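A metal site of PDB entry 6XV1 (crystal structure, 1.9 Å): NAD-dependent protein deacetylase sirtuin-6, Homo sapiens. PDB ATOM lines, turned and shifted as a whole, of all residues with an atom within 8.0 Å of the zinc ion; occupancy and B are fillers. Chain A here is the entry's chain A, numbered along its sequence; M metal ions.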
ATOM      1  N   GLU A 134      -1.987   4.981  16.282  1.00  0.00           N
ATOM      2  CA  GLU A 134      -2.780   6.045  16.916  1.00  0.00           C
ATOM      3  C   GLU A 134      -1.899   7.241  17.305  1.00  0.00           C
ATOM      4  O   GLU A 134      -0.856   7.036  17.866  1.00  0.00           O
ATOM      5  CB  GLU A 134      -3.454   5.428  18.137  1.00  0.00           C
ATOM      6  CG  GLU A 134      -4.325   6.381  18.902  1.00  0.00           C
ATOM      7  CD  GLU A 134      -5.098   5.706  20.006  1.00  0.00           C
ATOM      8  OE1 GLU A 134      -5.879   4.823  19.713  1.00  0.00           O
ATOM      9  OE2 GLU A 134      -4.904   6.050  21.148  1.00  0.00           O
ATOM     10  N   CYS A 135      -2.378   8.451  17.042  1.00  0.00           N
ATOM     11  CA  CYS A 135      -1.660   9.696  17.392  1.00  0.00           C
ATOM     12  C   CYS A 135      -1.741   9.922  18.911  1.00  0.00           C
ATOM     13  O   CYS A 135      -2.821  10.096  19.412  1.00  0.00           O
ATOM     14  CB  CYS A 135      -2.250  10.893  16.679  1.00  0.00           C
ATOM     15  SG  CYS A 135      -1.539  12.496  17.162  1.00  0.00           S
ATOM     16  N   ALA A 136      -0.600   9.869  19.573  1.00  0.00           N
ATOM     17  CA  ALA A 136      -0.473  10.163  21.026  1.00  0.00           C
ATOM     18  C   ALA A 136      -1.135  11.518  21.360  1.00  0.00           C
ATOM     19  O   ALA A 136      -1.796  11.624  22.422  1.00  0.00           O
ATOM     20  CB  ALA A 136       0.982  10.109  21.414  1.00  0.00           C
ATOM     21  N   LYS A 137      -1.074  12.526  20.482  1.00  0.00           N
ATOM     22  CA  LYS A 137      -1.639  13.877  20.780  1.00  0.00           C
ATOM     23  C   LYS A 137      -3.165  13.876  20.626  1.00  0.00           C
ATOM     24  O   LYS A 137      -3.819  14.145  21.640  1.00  0.00           O
ATOM     25  CB  LYS A 137      -0.945  14.981  19.957  1.00  0.00           C
ATOM     26  CG  LYS A 137       0.506  15.188  20.372  1.00  0.00           C
ATOM     27  CD  LYS A 137       1.051  16.596  20.249  1.00  0.00           C
ATOM     28  CE  LYS A 137       2.295  16.765  21.116  1.00  0.00           C
ATOM     29  NZ  LYS A 137       3.305  17.642  20.496  1.00  0.00           N
ATOM     30  N   CYS A 138      -3.707  13.622  19.433  1.00  0.00           N
ATOM     31  CA  CYS A 138      -5.128  13.938  19.098  1.00  0.00           C
ATOM     32  C   CYS A 138      -5.974  12.656  19.126  1.00  0.00           C
ATOM     33  O   CYS A 138      -7.177  12.779  18.947  1.00  0.00           O
ATOM     34  CB  CYS A 138      -5.255  14.660  17.756  1.00  0.00           C
ATOM     35  SG  CYS A 138      -4.752  13.646  16.327  1.00  0.00           S
ATOM     36  N   LYS A 139      -5.321  11.493  19.278  1.00  0.00           N
ATOM     37  CA  LYS A 139      -5.909  10.121  19.314  1.00  0.00           C
ATOM     38  C   LYS A 139      -6.482   9.720  17.955  1.00  0.00           C
ATOM     39  O   LYS A 139      -7.231   8.777  17.931  1.00  0.00           O
ATOM     40  CB  LYS A 139      -7.009  10.038  20.381  1.00  0.00           C
ATOM     41  CG  LYS A 139      -6.664  10.712  21.702  1.00  0.00           C
ATOM     42  CD  LYS A 139      -5.535  10.048  22.436  1.00  0.00           C
ATOM     43  CE  LYS A 139      -4.960  10.917  23.544  1.00  0.00           C
ATOM     44  NZ  LYS A 139      -3.984  10.168  24.375  1.00  0.00           N
ATOM     45  N   THR A 140      -6.127  10.372  16.839  1.00  0.00           N
ATOM     46  CA  THR A 140      -6.614   9.939  15.520  1.00  0.00           C
ATOM     47  C   THR A 140      -5.955   8.598  15.187  1.00  0.00           C
ATOM     48  O   THR A 140      -4.697   8.500  15.251  1.00  0.00           O
ATOM     49  CB  THR A 140      -6.364  10.944  14.401  1.00  0.00           C
ATOM     50  OG1 THR A 140      -7.050  12.163  14.683  1.00  0.00           O
ATOM     51  CG2 THR A 140      -6.800  10.401  13.045  1.00  0.00           C
ATOM     52  N   GLN A 141      -6.756   7.642  14.746  1.00  0.00           N
ATOM     53  CA  GLN A 141      -6.274   6.281  14.362  1.00  0.00           C
ATOM     54  C   GLN A 141      -6.161   6.215  12.847  1.00  0.00           C
ATOM     55  O   GLN A 141      -6.892   6.917  12.175  1.00  0.00           O
ATOM     56  CB  GLN A 141      -7.234   5.229  14.905  1.00  0.00           C
ATOM     57  CG  GLN A 141      -7.017   4.898  16.353  1.00  0.00           C
ATOM     58  CD  GLN A 141      -8.047   3.940  16.846  1.00  0.00           C
ATOM     59  OE1 GLN A 141      -9.085   3.690  16.212  1.00  0.00           O
ATOM     60  NE2 GLN A 141      -7.735   3.345  17.968  1.00  0.00           N
ATOM     61  N   TYR A 142      -5.146   5.543  12.358  1.00  0.00           N
ATOM     62  CA  TYR A 142      -4.911   5.287  10.927  1.00  0.00           C
ATOM     63  C   TYR A 142      -4.905   3.763  10.760  1.00  0.00           C
ATOM     64  O   TYR A 142      -4.217   3.105  11.546  1.00  0.00           O
ATOM     65  CB  TYR A 142      -3.567   5.868  10.495  1.00  0.00           C
ATOM     66  CG  TYR A 142      -3.391   7.339  10.738  1.00  0.00           C
ATOM     67  CD1 TYR A 142      -3.367   7.863  12.011  1.00  0.00           C
ATOM     68  CD2 TYR A 142      -3.343   8.219   9.667  1.00  0.00           C
ATOM     69  CE1 TYR A 142      -3.184   9.226  12.241  1.00  0.00           C
ATOM     70  CE2 TYR A 142      -3.137   9.583   9.863  1.00  0.00           C
ATOM     71  CZ  TYR A 142      -3.134  10.100  11.162  1.00  0.00           C
ATOM     72  OH  TYR A 142      -2.956  11.464  11.335  1.00  0.00           O
ATOM     73  N   LEU A 159       4.293  10.584  11.832  1.00  0.00           N
ATOM     74  CA  LEU A 159       3.644  11.719  12.503  1.00  0.00           C
ATOM     75  C   LEU A 159       2.232  11.861  11.968  1.00  0.00           C
ATOM     76  O   LEU A 159       1.959  11.469  10.803  1.00  0.00           O
ATOM     77  CB  LEU A 159       4.405  13.037  12.293  1.00  0.00           C
ATOM     78  CG  LEU A 159       5.822  13.130  12.828  1.00  0.00           C
ATOM     79  CD1 LEU A 159       6.267  14.591  12.764  1.00  0.00           C
ATOM     80  CD2 LEU A 159       5.957  12.560  14.242  1.00  0.00           C
ATOM     81  N   CYS A 160       1.413  12.497  12.783  1.00  0.00           N
ATOM     82  CA  CYS A 160      -0.005  12.715  12.563  1.00  0.00           C
ATOM     83  C   CYS A 160      -0.149  13.724  11.428  1.00  0.00           C
ATOM     84  O   CYS A 160       0.679  14.639  11.350  1.00  0.00           O
ATOM     85  CB  CYS A 160      -0.664  13.200  13.838  1.00  0.00           C
ATOM     86  SG  CYS A 160      -2.454  13.193  13.648  1.00  0.00           S
ATOM     87  N   THR A 161      -1.118  13.536  10.553  1.00  0.00           N
ATOM     88  CA  THR A 161      -1.287  14.445   9.403  1.00  0.00           C
ATOM     89  C   THR A 161      -2.640  15.111   9.532  1.00  0.00           C
ATOM     90  O   THR A 161      -3.084  15.640   8.553  1.00  0.00           O
ATOM     91  CB  THR A 161      -1.037  13.708   8.076  1.00  0.00           C
ATOM     92  OG1 THR A 161      -2.032  12.699   7.979  1.00  0.00           O
ATOM     93  CG2 THR A 161       0.350  13.116   7.932  1.00  0.00           C
ATOM     94  N   VAL A 162      -3.258  15.129  10.700  1.00  0.00           N
ATOM     95  CA  VAL A 162      -4.618  15.707  10.809  1.00  0.00           C
ATOM     96  C   VAL A 162      -4.535  17.230  10.564  1.00  0.00           C
ATOM     97  O   VAL A 162      -3.589  17.827  11.054  1.00  0.00           O
ATOM     98  CB  VAL A 162      -5.322  15.340  12.141  1.00  0.00           C
ATOM     99  CG1 VAL A 162      -6.473  16.298  12.444  1.00  0.00           C
ATOM    100  CG2 VAL A 162      -5.816  13.907  12.110  1.00  0.00           C
ATOM    101  N   ALA A 163      -5.482  17.766   9.766  1.00  0.00           N
ATOM    102  CA  ALA A 163      -5.706  19.176   9.349  1.00  0.00           C
ATOM    103  C   ALA A 163      -4.898  20.163  10.190  1.00  0.00           C
ATOM    104  O   ALA A 163      -5.377  20.480  11.299  1.00  0.00           O
ATOM    105  CB  ALA A 163      -7.188  19.506   9.407  1.00  0.00           C
ATOM    106  N   CYS A 171      -1.049  18.701  12.819  1.00  0.00           N
ATOM    107  CA  CYS A 171      -1.048  18.172  14.225  1.00  0.00           C
ATOM    108  C   CYS A 171       0.354  17.712  14.587  1.00  0.00           C
ATOM    109  O   CYS A 171       0.847  18.089  15.654  1.00  0.00           O
ATOM    110  CB  CYS A 171      -2.039  17.030  14.442  1.00  0.00           C
ATOM    111  SG  CYS A 171      -1.733  16.062  15.947  1.00  0.00           S
ATOM    112  N   ARG A 172       0.928  16.871  13.727  1.00  0.00           N
ATOM    113  CA  ARG A 172       2.288  16.309  13.810  1.00  0.00           C
ATOM    114  C   ARG A 172       2.518  15.555  15.130  1.00  0.00           C
ATOM    115  O   ARG A 172       3.710  15.300  15.436  1.00  0.00           O
ATOM    116  CB  ARG A 172       3.286  17.420  13.486  1.00  0.00           C
ATOM    117  CG  ARG A 172       3.181  17.882  12.040  1.00  0.00           C
ATOM    118  CD  ARG A 172       4.284  18.827  11.580  1.00  0.00           C
ATOM    119  NE  ARG A 172       5.232  19.068  12.661  1.00  0.00           N
ATOM    120  CZ  ARG A 172       6.417  18.467  12.835  1.00  0.00           C
ATOM    121  NH1 ARG A 172       6.852  17.554  11.996  1.00  0.00           N
ATOM    122  NH2 ARG A 172       7.153  18.788  13.876  1.00  0.00           N
ATOM    123  N   GLY A 173       1.453  15.029  15.750  1.00  0.00           N
ATOM    124  CA  GLY A 173       1.537  14.028  16.832  1.00  0.00           C
ATOM    125  C   GLY A 173       2.387  12.809  16.449  1.00  0.00           C
ATOM    126  O   GLY A 173       2.331  12.400  15.215  1.00  0.00           O
ATOM    127  N   GLU A 174       3.125  12.258  17.428  1.00  0.00           N
ATOM    128  CA  GLU A 174       3.835  10.942  17.363  1.00  0.00           C
ATOM    129  C   GLU A 174       2.792   9.806  17.228  1.00  0.00           C
ATOM    130  O   GLU A 174       1.890   9.698  18.117  1.00  0.00           O
ATOM    131  CB  GLU A 174       4.722  10.784  18.603  1.00  0.00           C
ATOM    132  CG  GLU A 174       5.548   9.500  18.655  1.00  0.00           C
ATOM    133  CD  GLU A 174       6.493   9.415  19.861  1.00  0.00           C
ATOM    134  OE1 GLU A 174       7.531  10.090  19.815  1.00  0.00           O
ATOM    135  OE2 GLU A 174       6.218   8.658  20.821  1.00  0.00           O
ATOM    136  N   LEU A 175       2.852   9.043  16.126  1.00  0.00           N
ATOM    137  CA  LEU A 175       2.078   7.801  15.934  1.00  0.00           C
ATOM    138  C   LEU A 175       2.711   6.710  16.798  1.00  0.00           C
ATOM    139  O   LEU A 175       3.952   6.684  16.972  1.00  0.00           O
ATOM    140  CB  LEU A 175       1.977   7.463  14.445  1.00  0.00           C
ATOM    141  CG  LEU A 175       1.318   8.568  13.601  1.00  0.00           C
ATOM    142  CD1 LEU A 175       0.812   8.043  12.290  1.00  0.00           C
ATOM    143  CD2 LEU A 175       0.194   9.195  14.385  1.00  0.00           C
HETATM  144 ZN    ZN M   1      -2.778  13.895  15.891  1.00  0.00          ZN
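The backbone NH (N) of Cys 171 lies within hydrogen-bond range of the backbone carbonyl oxygen (O) of Val 162. N of Gly 173 lies close to SG of Cys 171, at 3.4 Å. The side-chain hydroxyl (OH) of Tyr 142 sits close to the side-chain sulfur (SG) of Cys 160, at 2.9 Å. The backbone carbonyl oxygen (O) of Cys 160 lies within hydrogen-bond range of the backbone NH (N) of Arg 172. The backbone carbonyl oxygen of Thr 140 lies within hydrogen-bond range of the backbone NH of Cys 135, at 2.9 Å. N of Cys 160 lies within hydrogen-bond range of O of Gly 173, at 2.6 Å. SG of Cys 135 lies close to N of Lys 137 (3.4 Å). OG1 of Thr 140 lies close to SG of Cys 138, 3.2 Å away.
The nearest printed residue that does not touch the zinc ion is Gly 173 (4.4 Å).
The zinc ion is bound by the side-chain sulfur (SG) of Cys 138, at 2.0 Å. SG of Cys 135 is bound to the zinc ion (2.3 Å). The zinc ion is bound by SG of Cys 160. SG of Cys 171 is bound to the zinc ion (2.4 Å).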
